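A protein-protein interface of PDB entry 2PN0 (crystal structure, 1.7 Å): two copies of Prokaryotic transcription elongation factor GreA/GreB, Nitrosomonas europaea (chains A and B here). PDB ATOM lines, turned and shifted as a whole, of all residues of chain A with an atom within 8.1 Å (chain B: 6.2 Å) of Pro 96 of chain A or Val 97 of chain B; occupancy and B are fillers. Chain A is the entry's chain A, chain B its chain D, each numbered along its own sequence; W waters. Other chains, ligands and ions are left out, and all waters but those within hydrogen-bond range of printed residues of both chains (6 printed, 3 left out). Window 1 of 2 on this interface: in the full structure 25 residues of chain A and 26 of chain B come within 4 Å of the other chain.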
ATOM      1  N   PHE A  31      -6.981  -1.813  19.060  1.00  0.00           N
ATOM      2  CA  PHE A  31      -8.298  -2.262  18.565  1.00  0.00           C
ATOM      3  C   PHE A  31      -8.810  -3.405  19.465  1.00  0.00           C
ATOM      4  O   PHE A  31      -8.003  -4.099  20.121  1.00  0.00           O
ATOM      5  CB  PHE A  31      -8.269  -2.659  17.076  1.00  0.00           C
ATOM      6  CG  PHE A  31      -7.306  -3.798  16.750  1.00  0.00           C
ATOM      7  CD1 PHE A  31      -7.702  -5.121  16.863  1.00  0.00           C
ATOM      8  CD2 PHE A  31      -6.006  -3.521  16.340  1.00  0.00           C
ATOM      9  CE1 PHE A  31      -6.825  -6.158  16.560  1.00  0.00           C
ATOM     10  CE2 PHE A  31      -5.118  -4.567  16.039  1.00  0.00           C
ATOM     11  CZ  PHE A  31      -5.541  -5.876  16.158  1.00  0.00           C
ATOM     12  N   PRO A  32     -10.130  -3.595  19.522  1.00  0.00           N
ATOM     13  CA  PRO A  32     -10.636  -4.589  20.480  1.00  0.00           C
ATOM     14  C   PRO A  32     -10.120  -5.989  20.174  1.00  0.00           C
ATOM     15  O   PRO A  32     -10.111  -6.409  19.014  1.00  0.00           O
ATOM     16  CB  PRO A  32     -12.156  -4.525  20.291  1.00  0.00           C
ATOM     17  CG  PRO A  32     -12.369  -3.851  18.907  1.00  0.00           C
ATOM     18  CD  PRO A  32     -11.211  -2.897  18.787  1.00  0.00           C
ATOM     19  N   GLY A  33      -9.663  -6.696  21.201  1.00  0.00           N
ATOM     20  CA  GLY A  33      -9.182  -8.072  21.004  1.00  0.00           C
ATOM     21  C   GLY A  33      -7.755  -8.153  20.470  1.00  0.00           C
ATOM     22  O   GLY A  33      -7.250  -9.266  20.205  1.00  0.00           O
ATOM     23  N   LEU A  76     -18.976 -14.421   4.685  1.00  0.00           N
ATOM     24  CA  LEU A  76     -18.002 -13.359   4.917  1.00  0.00           C
ATOM     25  C   LEU A  76     -16.623 -13.851   4.468  1.00  0.00           C
ATOM     26  O   LEU A  76     -16.219 -14.974   4.804  1.00  0.00           O
ATOM     27  CB  LEU A  76     -17.963 -12.963   6.399  1.00  0.00           C
ATOM     28  CG  LEU A  76     -19.185 -12.318   7.069  1.00  0.00           C
ATOM     29  CD1 LEU A  76     -19.063 -12.303   8.577  1.00  0.00           C
ATOM     30  CD2 LEU A  76     -19.482 -10.911   6.552  1.00  0.00           C
ATOM     31  N   ILE A  91     -14.796  -8.862   5.626  1.00  0.00           N
ATOM     32  CA  ILE A  91     -14.605  -8.490   7.002  1.00  0.00           C
ATOM     33  C   ILE A  91     -13.119  -8.462   7.306  1.00  0.00           C
ATOM     34  O   ILE A  91     -12.403  -9.451   7.090  1.00  0.00           O
ATOM     35  CB  ILE A  91     -15.438  -9.400   7.989  1.00  0.00           C
ATOM     36  CG1 ILE A  91     -15.449  -8.789   9.402  1.00  0.00           C
ATOM     37  CG2 ILE A  91     -14.985 -10.863   7.956  1.00  0.00           C
ATOM     38  CD1 ILE A  91     -16.545  -9.436  10.281  1.00  0.00           C
ATOM     39  N   SER A  92     -12.668  -7.322   7.830  1.00  0.00           N
ATOM     40  CA  SER A  92     -11.241  -7.176   8.184  1.00  0.00           C
ATOM     41  C   SER A  92     -10.827  -8.086   9.346  1.00  0.00           C
ATOM     42  O   SER A  92     -11.573  -8.237  10.328  1.00  0.00           O
ATOM     43  CB  SER A  92     -10.914  -5.708   8.540  1.00  0.00           C
ATOM     44  OG  SER A  92      -9.571  -5.528   8.953  1.00  0.00           O
ATOM     45  N   ILE A  93      -9.588  -8.555   9.287  1.00  0.00           N
ATOM     46  CA  ILE A  93      -8.941  -9.203  10.424  1.00  0.00           C
ATOM     47  C   ILE A  93      -8.894  -8.291  11.655  1.00  0.00           C
ATOM     48  O   ILE A  93      -8.793  -8.793  12.774  1.00  0.00           O
ATOM     49  CB  ILE A  93      -7.513  -9.699  10.021  1.00  0.00           C
ATOM     50  CG1 ILE A  93      -6.869 -10.556  11.113  1.00  0.00           C
ATOM     51  CG2 ILE A  93      -6.616  -8.530   9.571  1.00  0.00           C
ATOM     52  CD1 ILE A  93      -7.652 -11.811  11.526  1.00  0.00           C
ATOM     53  N   LEU A  94      -8.996  -6.977  11.455  1.00  0.00           N
ATOM     54  CA  LEU A  94      -8.971  -5.991  12.603  1.00  0.00           C
ATOM     55  C   LEU A  94     -10.342  -5.766  13.237  1.00  0.00           C
ATOM     56  O   LEU A  94     -10.428  -5.176  14.310  1.00  0.00           O
ATOM     57  CB  LEU A  94      -8.391  -4.625  12.182  1.00  0.00           C
ATOM     58  CG  LEU A  94      -7.035  -4.702  11.472  1.00  0.00           C
ATOM     59  CD1 LEU A  94      -6.581  -3.256  11.259  1.00  0.00           C
ATOM     60  CD2 LEU A  94      -6.034  -5.455  12.309  1.00  0.00           C
ATOM     61  N   ALA A  95     -11.402  -6.223  12.575  1.00  0.00           N
ATOM     62  CA  ALA A  95     -12.767  -5.875  13.016  1.00  0.00           C
ATOM     63  C   ALA A  95     -13.294  -6.873  14.060  1.00  0.00           C
ATOM     64  O   ALA A  95     -12.935  -8.072  14.006  1.00  0.00           O
ATOM     65  CB  ALA A  95     -13.722  -5.815  11.831  1.00  0.00           C
ATOM     66  N   PRO A  96     -14.195  -6.421  14.958  1.00  0.00           N
ATOM     67  CA  PRO A  96     -14.934  -7.371  15.779  1.00  0.00           C
ATOM     68  C   PRO A  96     -15.496  -8.492  14.876  1.00  0.00           C
ATOM     69  O   PRO A  96     -15.957  -8.231  13.729  1.00  0.00           O
ATOM     70  CB  PRO A  96     -16.071  -6.533  16.362  1.00  0.00           C
ATOM     71  CG  PRO A  96     -15.436  -5.142  16.508  1.00  0.00           C
ATOM     72  CD  PRO A  96     -14.542  -5.017  15.269  1.00  0.00           C
ATOM     73  N   VAL A  97     -15.423  -9.703  15.393  1.00  0.00           N
ATOM     74  CA  VAL A  97     -15.786 -10.949  14.646  1.00  0.00           C
ATOM     75  C   VAL A  97     -14.684 -11.366  13.697  1.00  0.00           C
ATOM     76  O   VAL A  97     -14.180 -12.492  13.816  1.00  0.00           O
ATOM     77  CB  VAL A  97     -17.174 -10.943  13.939  1.00  0.00           C
ATOM     78  CG1 VAL A  97     -17.409 -12.317  13.268  1.00  0.00           C
ATOM     79  CG2 VAL A  97     -18.280 -10.699  14.966  1.00  0.00           C
ATOM     80  N   GLY A  98     -14.306 -10.456  12.782  1.00  0.00           N
ATOM     81  CA  GLY A  98     -13.205 -10.697  11.837  1.00  0.00           C
ATOM     82  C   GLY A  98     -11.955 -11.208  12.572  1.00  0.00           C
ATOM     83  O   GLY A  98     -11.358 -12.245  12.193  1.00  0.00           O
ATOM     84  N   SER A  99     -11.541 -10.513  13.630  1.00  0.00           N
ATOM     85  CA  SER A  99     -10.336 -10.921  14.382  1.00  0.00           C
ATOM     86  C   SER A  99     -10.473 -12.305  14.998  1.00  0.00           C
ATOM     87  O   SER A  99      -9.469 -12.948  15.256  1.00  0.00           O
ATOM     88  CB  SER A  99      -9.967  -9.872  15.469  1.00  0.00           C
ATOM     89  OG  SER A  99     -11.043  -9.667  16.393  1.00  0.00           O
ATOM     90  N   ALA A 100     -11.698 -12.740  15.280  1.00  0.00           N
ATOM     91  CA  ALA A 100     -11.925 -14.079  15.872  1.00  0.00           C
ATOM     92  C   ALA A 100     -12.080 -15.178  14.813  1.00  0.00           C
ATOM     93  O   ALA A 100     -12.062 -16.377  15.155  1.00  0.00           O
ATOM     94  CB  ALA A 100     -13.208 -14.043  16.766  1.00  0.00           C
ATOM     95  N   LEU A 101     -12.278 -14.813  13.548  1.00  0.00           N
ATOM     96  CA  LEU A 101     -12.546 -15.861  12.535  1.00  0.00           C
ATOM     97  C   LEU A 101     -11.293 -16.659  12.183  1.00  0.00           C
ATOM     98  O   LEU A 101     -11.390 -17.835  11.853  1.00  0.00           O
ATOM     99  CB  LEU A 101     -13.143 -15.279  11.226  1.00  0.00           C
ATOM    100  CG  LEU A 101     -14.582 -14.788  11.276  1.00  0.00           C
ATOM    101  CD1 LEU A 101     -14.982 -14.158   9.898  1.00  0.00           C
ATOM    102  CD2 LEU A 101     -15.577 -15.930  11.653  1.00  0.00           C
ATOM    103  N   GLU A 111     -21.114 -16.469  17.835  1.00  0.00           N
ATOM    104  CA  GLU A 111     -22.298 -15.641  17.920  1.00  0.00           C
ATOM    105  C   GLU A 111     -21.904 -14.171  18.101  1.00  0.00           C
ATOM    106  O   GLU A 111     -20.804 -13.849  18.603  1.00  0.00           O
ATOM    107  CB  GLU A 111     -23.233 -16.140  19.052  1.00  0.00           C
ATOM    108  CG  GLU A 111     -22.668 -15.961  20.425  1.00  0.00           C
ATOM    109  CD  GLU A 111     -23.512 -16.644  21.501  1.00  0.00           C
ATOM    110  OE1 GLU A 111     -24.218 -17.668  21.232  1.00  0.00           O
ATOM    111  OE2 GLU A 111     -23.418 -16.143  22.616  1.00  0.00           O
ATOM    112  N   TRP A 112     -22.792 -13.282  17.689  1.00  0.00           N
ATOM    113  CA  TRP A 112     -22.529 -11.871  17.888  1.00  0.00           C
ATOM    114  C   TRP A 112     -23.848 -11.155  18.057  1.00  0.00           C
ATOM    115  O   TRP A 112     -24.925 -11.767  17.871  1.00  0.00           O
ATOM    116  CB  TRP A 112     -21.634 -11.294  16.794  1.00  0.00           C
ATOM    117  CG  TRP A 112     -22.169 -11.317  15.381  1.00  0.00           C
ATOM    118  CD1 TRP A 112     -23.100 -10.442  14.824  1.00  0.00           C
ATOM    119  CD2 TRP A 112     -21.798 -12.229  14.335  1.00  0.00           C
ATOM    120  NE1 TRP A 112     -23.307 -10.782  13.484  1.00  0.00           N
ATOM    121  CE2 TRP A 112     -22.510 -11.849  13.167  1.00  0.00           C
ATOM    122  CE3 TRP A 112     -20.902 -13.314  14.261  1.00  0.00           C
ATOM    123  CZ2 TRP A 112     -22.374 -12.539  11.918  1.00  0.00           C
ATOM    124  CZ3 TRP A 112     -20.750 -14.004  12.987  1.00  0.00           C
ATOM    125  CH2 TRP A 112     -21.471 -13.589  11.857  1.00  0.00           C
ATOM    126  N   PRO A 113     -23.790  -9.878  18.457  1.00  0.00           N
ATOM    127  CA  PRO A 113     -25.066  -9.240  18.793  1.00  0.00           C
ATOM    128  C   PRO A 113     -26.118  -9.093  17.658  1.00  0.00           C
ATOM    129  O   PRO A 113     -25.762  -8.823  16.497  1.00  0.00           O
ATOM    130  CB  PRO A 113     -24.641  -7.845  19.276  1.00  0.00           C
ATOM    131  CG  PRO A 113     -23.237  -8.043  19.746  1.00  0.00           C
ATOM    132  CD  PRO A 113     -22.642  -8.983  18.709  1.00  0.00           C
ATOM    133  N   LYS A 114     -27.390  -9.298  18.019  1.00  0.00           N
ATOM    134  CA  LYS A 114     -28.509  -8.956  17.144  1.00  0.00           C
ATOM    135  C   LYS A 114     -28.899  -7.480  17.388  1.00  0.00           C
ATOM    136  O   LYS A 114     -29.059  -7.070  18.523  1.00  0.00           O
ATOM    137  CB  LYS A 114     -29.736  -9.852  17.439  1.00  0.00           C
ATOM    138  CG  LYS A 114     -29.589 -11.230  16.844  1.00  0.00           C
ATOM    139  CD  LYS A 114     -30.809 -12.132  17.083  1.00  0.00           C
ATOM    140  CE  LYS A 114     -32.100 -11.425  17.211  1.00  0.00           C
ATOM    141  NZ  LYS A 114     -33.074 -12.550  17.484  1.00  0.00           N
ATOM    142  N   PRO A 115     -29.081  -6.684  16.323  1.00  0.00           N
ATOM    143  CA  PRO A 115     -29.615  -5.317  16.515  1.00  0.00           C
ATOM    144  C   PRO A 115     -30.925  -5.342  17.284  1.00  0.00           C
ATOM    145  O   PRO A 115     -31.816  -6.143  16.952  1.00  0.00           O
ATOM    146  CB  PRO A 115     -29.812  -4.804  15.084  1.00  0.00           C
ATOM    147  CG  PRO A 115     -28.858  -5.647  14.251  1.00  0.00           C
ATOM    148  CD  PRO A 115     -28.841  -7.001  14.915  1.00  0.00           C
ATOM    149  N   PHE B  65     -15.460   1.991  24.824  1.00  0.00           N
ATOM    150  CA  PHE B  65     -15.848   0.789  25.540  1.00  0.00           C
ATOM    151  C   PHE B  65     -14.837   0.430  26.622  1.00  0.00           C
ATOM    152  O   PHE B  65     -13.627   0.623  26.443  1.00  0.00           O
ATOM    153  CB  PHE B  65     -15.872  -0.395  24.595  1.00  0.00           C
ATOM    154  CG  PHE B  65     -16.800  -0.234  23.449  1.00  0.00           C
ATOM    155  CD1 PHE B  65     -18.090  -0.761  23.505  1.00  0.00           C
ATOM    156  CD2 PHE B  65     -16.358   0.417  22.282  1.00  0.00           C
ATOM    157  CE1 PHE B  65     -18.960  -0.631  22.398  1.00  0.00           C
ATOM    158  CE2 PHE B  65     -17.228   0.547  21.171  1.00  0.00           C
ATOM    159  CZ  PHE B  65     -18.504   0.026  21.240  1.00  0.00           C
ATOM    160  N   LEU B  76     -14.632   2.643  19.028  1.00  0.00           N
ATOM    161  CA  LEU B  76     -15.073   2.403  17.655  1.00  0.00           C
ATOM    162  C   LEU B  76     -16.002   3.533  17.223  1.00  0.00           C
ATOM    163  O   LEU B  76     -16.860   3.927  17.992  1.00  0.00           O
ATOM    164  CB  LEU B  76     -15.898   1.121  17.532  1.00  0.00           C
ATOM    165  CG  LEU B  76     -15.136  -0.180  17.804  1.00  0.00           C
ATOM    166  CD1 LEU B  76     -16.157  -1.293  17.914  1.00  0.00           C
ATOM    167  CD2 LEU B  76     -14.043  -0.508  16.712  1.00  0.00           C
ATOM    168  N   LEU B  78     -18.924   4.557  14.655  1.00  0.00           N
ATOM    169  CA  LEU B  78     -19.963   3.906  13.847  1.00  0.00           C
ATOM    170  C   LEU B  78     -20.190   4.707  12.594  1.00  0.00           C
ATOM    171  O   LEU B  78     -20.570   5.896  12.677  1.00  0.00           O
ATOM    172  CB  LEU B  78     -21.279   3.861  14.651  1.00  0.00           C
ATOM    173  CG  LEU B  78     -22.452   3.145  13.949  1.00  0.00           C
ATOM    174  CD1 LEU B  78     -22.119   1.685  13.485  1.00  0.00           C
ATOM    175  CD2 LEU B  78     -23.675   3.219  14.886  1.00  0.00           C
ATOM    176  N   GLY B  88      -8.674  -0.116  12.144  1.00  0.00           N
ATOM    177  CA  GLY B  88      -9.328  -0.788  13.251  1.00  0.00           C
ATOM    178  C   GLY B  88     -10.185   0.106  14.125  1.00  0.00           C
ATOM    179  O   GLY B  88     -10.684  -0.382  15.146  1.00  0.00           O
ATOM    180  N   ILE B  91     -16.231   1.292  12.289  1.00  0.00           N
ATOM    181  CA  ILE B  91     -17.008   0.077  12.079  1.00  0.00           C
ATOM    182  C   ILE B  91     -18.290   0.405  11.303  1.00  0.00           C
ATOM    183  O   ILE B  91     -19.005   1.372  11.636  1.00  0.00           O
ATOM    184  CB  ILE B  91     -17.289  -0.639  13.421  1.00  0.00           C
ATOM    185  CG1 ILE B  91     -17.818  -2.083  13.161  1.00  0.00           C
ATOM    186  CG2 ILE B  91     -18.245   0.203  14.319  1.00  0.00           C
ATOM    187  CD1 ILE B  91     -17.927  -2.968  14.454  1.00  0.00           C
ATOM    188  N   SER B  92     -18.568  -0.374  10.254  1.00  0.00           N
ATOM    189  CA  SER B  92     -19.754  -0.131   9.426  1.00  0.00           C
ATOM    190  C   SER B  92     -21.056  -0.473  10.155  1.00  0.00           C
ATOM    191  O   SER B  92     -21.103  -1.469  10.884  1.00  0.00           O
ATOM    192  CB  SER B  92     -19.666  -0.908   8.098  1.00  0.00           C
ATOM    193  OG  SER B  92     -20.839  -0.717   7.359  1.00  0.00           O
ATOM    194  N   ALA B  95     -21.903  -3.993   9.555  1.00  0.00           N
ATOM    195  CA  ALA B  95     -20.985  -5.003  10.033  1.00  0.00           C
ATOM    196  C   ALA B  95     -21.535  -5.740  11.242  1.00  0.00           C
ATOM    197  O   ALA B  95     -22.316  -5.167  12.012  1.00  0.00           O
ATOM    198  CB  ALA B  95     -19.636  -4.360  10.421  1.00  0.00           C
ATOM    199  N   PRO B  96     -21.080  -6.996  11.474  1.00  0.00           N
ATOM    200  CA  PRO B  96     -21.345  -7.603  12.792  1.00  0.00           C
ATOM    201  C   PRO B  96     -20.811  -6.634  13.870  1.00  0.00           C
ATOM    202  O   PRO B  96     -19.772  -5.982  13.665  1.00  0.00           O
ATOM    203  CB  PRO B  96     -20.470  -8.865  12.766  1.00  0.00           C
ATOM    204  CG  PRO B  96     -20.500  -9.251  11.232  1.00  0.00           C
ATOM    205  CD  PRO B  96     -20.263  -7.888  10.621  1.00  0.00           C
ATOM    206  N   VAL B  97     -21.586  -6.510  14.940  1.00  0.00           N
ATOM    207  CA  VAL B  97     -21.382  -5.558  16.036  1.00  0.00           C
ATOM    208  C   VAL B  97     -21.840  -4.174  15.654  1.00  0.00           C
ATOM    209  O   VAL B  97     -22.706  -3.609  16.336  1.00  0.00           O
ATOM    210  CB  VAL B  97     -19.943  -5.611  16.637  1.00  0.00           C
ATOM    211  CG1 VAL B  97     -19.760  -4.530  17.770  1.00  0.00           C
ATOM    212  CG2 VAL B  97     -19.651  -7.020  17.141  1.00  0.00           C
ATOM    213  N   GLY B  98     -21.296  -3.642  14.562  1.00  0.00           N
ATOM    214  CA  GLY B  98     -21.700  -2.293  14.089  1.00  0.00           C
ATOM    215  C   GLY B  98     -23.239  -2.178  14.020  1.00  0.00           C
ATOM    216  O   GLY B  98     -23.839  -1.203  14.506  1.00  0.00           O
ATOM    217  N   SER B  99     -23.885  -3.169  13.430  1.00  0.00           N
ATOM    218  CA  SER B  99     -25.340  -3.068  13.236  1.00  0.00           C
ATOM    219  C   SER B  99     -26.093  -2.995  14.572  1.00  0.00           C
ATOM    220  O   SER B  99     -27.187  -2.403  14.656  1.00  0.00           O
ATOM    221  CB  SER B  99     -25.836  -4.225  12.348  1.00  0.00           C
ATOM    222  OG  SER B  99     -25.541  -5.510  12.950  1.00  0.00           O
ATOM    223  N   ALA B 100     -25.540  -3.640  15.599  1.00  0.00           N
ATOM    224  CA  ALA B 100     -26.153  -3.603  16.937  1.00  0.00           C
ATOM    225  C   ALA B 100     -25.807  -2.357  17.775  1.00  0.00           C
ATOM    226  O   ALA B 100     -26.433  -2.113  18.816  1.00  0.00           O
ATOM    227  CB  ALA B 100     -25.772  -4.848  17.693  1.00  0.00           C
ATOM    228  N   LEU B 101     -24.755  -1.620  17.394  1.00  0.00           N
ATOM    229  CA  LEU B 101     -24.340  -0.459  18.209  1.00  0.00           C
ATOM    230  C   LEU B 101     -25.370   0.675  18.115  1.00  0.00           C
ATOM    231  O   LEU B 101     -25.581   1.389  19.101  1.00  0.00           O
ATOM    232  CB  LEU B 101     -22.963   0.089  17.769  1.00  0.00           C
ATOM    233  CG  LEU B 101     -21.796  -0.812  18.178  1.00  0.00           C
ATOM    234  CD1 LEU B 101     -20.526  -0.127  17.635  1.00  0.00           C
ATOM    235  CD2 LEU B 101     -21.687  -0.869  19.728  1.00  0.00           C
ATOM    236  N   LEU B 102     -25.986   0.804  16.946  1.00  0.00           N
ATOM    237  CA  LEU B 102     -26.867   1.966  16.672  1.00  0.00           C
ATOM    238  C   LEU B 102     -27.968   2.015  17.738  1.00  0.00           C
ATOM    239  O   LEU B 102     -28.638   1.017  17.976  1.00  0.00           O
ATOM    240  CB  LEU B 102     -27.502   1.861  15.301  1.00  0.00           C
ATOM    241  CG  LEU B 102     -28.339   3.066  14.915  1.00  0.00           C
ATOM    242  CD1 LEU B 102     -27.505   4.347  14.783  1.00  0.00           C
ATOM    243  CD2 LEU B 102     -29.106   2.796  13.630  1.00  0.00           C
ATOM    244  N   ILE B 110     -22.415  -5.049  25.737  1.00  0.00           N
ATOM    245  CA  ILE B 110     -22.453  -5.744  24.493  1.00  0.00           C
ATOM    246  C   ILE B 110     -21.296  -6.733  24.526  1.00  0.00           C
ATOM    247  O   ILE B 110     -20.343  -6.529  25.256  1.00  0.00           O
ATOM    248  CB  ILE B 110     -22.380  -4.709  23.292  1.00  0.00           C
ATOM    249  CG1 ILE B 110     -22.316  -5.365  21.937  1.00  0.00           C
ATOM    250  CG2 ILE B 110     -21.223  -3.758  23.433  1.00  0.00           C
ATOM    251  CD1 ILE B 110     -22.570  -4.344  20.814  1.00  0.00           C
ATOM    252  N   GLU B 111     -21.402  -7.811  23.770  1.00  0.00           N
ATOM    253  CA  GLU B 111     -20.324  -8.794  23.773  1.00  0.00           C
ATOM    254  C   GLU B 111     -20.176  -9.410  22.403  1.00  0.00           C
ATOM    255  O   GLU B 111     -21.139  -9.488  21.604  1.00  0.00           O
ATOM    256  CB  GLU B 111     -20.563  -9.892  24.835  1.00  0.00           C
ATOM    257  CG  GLU B 111     -21.873 -10.620  24.701  1.00  0.00           C
ATOM    258  CD  GLU B 111     -22.026 -11.666  25.805  1.00  0.00           C
ATOM    259  OE1 GLU B 111     -21.922 -11.303  27.014  1.00  0.00           O
ATOM    260  OE2 GLU B 111     -22.209 -12.849  25.466  1.00  0.00           O
ATOM    261  N   TRP B 112     -18.983  -9.907  22.120  1.00  0.00           N
ATOM    262  CA  TRP B 112     -18.737 -10.493  20.825  1.00  0.00           C
ATOM    263  C   TRP B 112     -17.540 -11.454  20.920  1.00  0.00           C
ATOM    264  O   TRP B 112     -16.874 -11.474  21.954  1.00  0.00           O
ATOM    265  CB  TRP B 112     -18.592  -9.432  19.697  1.00  0.00           C
ATOM    266  CG  TRP B 112     -17.440  -8.442  19.863  1.00  0.00           C
ATOM    267  CD1 TRP B 112     -16.142  -8.685  19.623  1.00  0.00           C
ATOM    268  CD2 TRP B 112     -17.529  -7.084  20.315  1.00  0.00           C
ATOM    269  NE1 TRP B 112     -15.379  -7.544  19.831  1.00  0.00           N
ATOM    270  CE2 TRP B 112     -16.205  -6.547  20.275  1.00  0.00           C
ATOM    271  CE3 TRP B 112     -18.588  -6.244  20.673  1.00  0.00           C
ATOM    272  CZ2 TRP B 112     -15.911  -5.217  20.626  1.00  0.00           C
ATOM    273  CZ3 TRP B 112     -18.292  -4.929  21.059  1.00  0.00           C
ATOM    274  CH2 TRP B 112     -16.964  -4.415  20.989  1.00  0.00           C
ATOM    275  N   PRO B 113     -17.307 -12.265  19.872  1.00  0.00           N
ATOM    276  CA  PRO B 113     -16.245 -13.270  20.000  1.00  0.00           C
ATOM    277  C   PRO B 113     -14.849 -12.701  20.257  1.00  0.00           C
ATOM    278  O   PRO B 113     -14.402 -11.775  19.553  1.00  0.00           O
ATOM    279  CB  PRO B 113     -16.253 -13.976  18.634  1.00  0.00           C
ATOM    280  CG  PRO B 113     -17.612 -13.737  18.103  1.00  0.00           C
ATOM    281  CD  PRO B 113     -17.950 -12.351  18.543  1.00  0.00           C
HETATM  282  O   HOH W   1     -13.529 -10.275  17.467  1.00  0.00           O
HETATM  283  O   HOH W   2     -17.285  -6.196  12.438  1.00  0.00           O
HETATM  284  O   HOH W   3     -24.375  -6.849  15.221  1.00  0.00           O
HETATM  285  O   HOH W   4     -11.843  -2.907  15.078  1.00  0.00           O
HETATM  286  O   HOH W   5     -22.171 -13.628  22.796  1.00  0.00           O
HETATM  287  O   HOH W   6     -12.501  -8.103  19.239  1.00  0.00           O
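The side-chain hydroxyl (OG) of Ser 92 of chain A is in hydrogen-bond range of the backbone NH (N) of Leu 94 of chain A (2.9 Å). The backbone carbonyl oxygen of Ala 95 of chain B is in hydrogen-bond range of the side-chain hydroxyl of Ser 99 of chain B, 3.4 Å away.
Phe 31 of chain A touches Gly 88 of chain B. Pro 32 of chain A touches Trp 112 of chain B. Val 97 of chain B touches Pro 96 of chain A (CG2 to CB, 3.7 Å). Pro 96 of chain A touches Trp 112 of chain B. CG2 of Val 97 of chain A touches CB of Pro 96 of chain B, 3.6 Å away. Pro 113 of chain B touches Val 97 of chain A. Pro 113 of chain B touches Glu 111 of chain A. CB of Pro 113 of chain A touches CB of Ala 100 of chain B, at 3.6 Å. O of Glu 111 of chain B touches CG of Pro 113 of chain A, 3.2 Å away. CA of Pro 115 of chain A touches CA of Ala 100 of chain B, 3.9 Å away.
Of the printed residues of chain B, Phe 31 of chain A touches Gly 88. Gly 33 of chain A touches none of the printed residues of chain B. Pro 96 of chain A touches three residues of chain B. Printed residues of chain B within 4 Å of Glu 111 of chain A: Pro 113. Of chain A, only Pro 96 (3.7 Å) and Pro 113 (3.9 Å) come within 4 Å of Val 97 of chain B. No residue of chain A comes within 4 Å of Gly 98 of chain B. Of the printed residues of chain A, Ser 99 of chain B touches Pro 115 (3.6 Å). Printed residues of chain A within 4 Å of Ile 110 of chain B: Pro 113. Printed residues of chain A within 4 Å of Glu 111 of chain B: Pro 113 (3.2 Å). The nearest residue of chain B that does not touch Pro 96 of chain A is Leu 76 of chain B (4.2 Å). The nearest printed residue of chain A that does not touch Ile 110 of chain B is Trp 112 of chain A (7.1 Å).
Of the 20 printed residues of chain A, 10 touch a printed residue of chain B. Printed residues of chain A that touch a printed residue of chain B: Phe 31, Pro 32, Leu 94, Pro 96, Val 97, Ala 100, Glu 111, Trp 112, Pro 113 and Pro 115. Hydrophobic or aromatic side chains of chain A within 4 Å of the printed part of chain B: Phe 31, Pro 32, Leu 94, Pro 96, Val 97, Ala 100, Trp 112, Pro 113 and Pro 115. Along chain A the printed residues that touch a printed residue of chain B span positions 31 to 115. Printed residues of chain B that touch a printed residue of chain A: Gly 88, Ile 91, Pro 96, Val 97, Ser 99, Ala 100, Ile 110, Glu 111, Trp 112 and Pro 113. Hydrophobic or aromatic side chains of chain B that line the printed part of chain A: Ile 91, Pro 96, Val 97, Ala 100, Ile 110, Trp 112 and Pro 113. Among the printed residues, 17 pairs touch across the chains.
Pro 96 of chain A touches Val 97 of chain B, and with the chains exchanged Val 97 of chain A touches Pro 96 of chain B. Pro 96 of chain A touches Trp 112 of chain B, and with the chains exchanged Trp 112 of chain A touches Pro 96 of chain B. Val 97 of chain A touches Pro 113 of chain B, and with the chains exchanged Pro 113 of chain A touches Val 97 of chain B. Glu 111 of chain A touches Pro 113 of chain B, and with the chains exchanged Pro 113 of chain A touches Glu 111 of chain B. Positions printed for both chains: 76, 91, 92, 95, 96, 97, 98, 99, 100, 101, 111, 112 and 113. Of the 17 pairs that touch across the chains among the printed residues, 10 have their exchanged pair printed and touching as well.
Water W1 lies within hydrogen-bond range of O of Pro 113 of chain B, OG of Ser 99 of chain A and N of Val 97 of chain A. Water W3 lies within hydrogen-bond range of O of Pro 113 of chain A (2.7 Å), N of Val 97 of chain B (2.8 Å), OG of Ser 99 of chain B (2.9 Å) and N of Ala 100 of chain B (3.4 Å). Water W2 lies within hydrogen-bond range of O of Pro 96 of chain A (2.8 Å) and O of Pro 96 of chain B (2.8 Å). Water W4 lies within hydrogen-bond range of the backbone carbonyl oxygen of Gly 88 of chain B and the backbone carbonyl oxygen of Leu 94 of chain A. Water W5 bridges the side-chain carboxylate (OE2) of Glu 111 of chain B (2.8 Å) and the side-chain carboxylate (OE2) of Glu 111 of chain A (2.8 Å). Water W6 bridges O of Pro 32 of chain A (2.9 Å) and NE1 of Trp 112 of chain B (3.0 Å).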
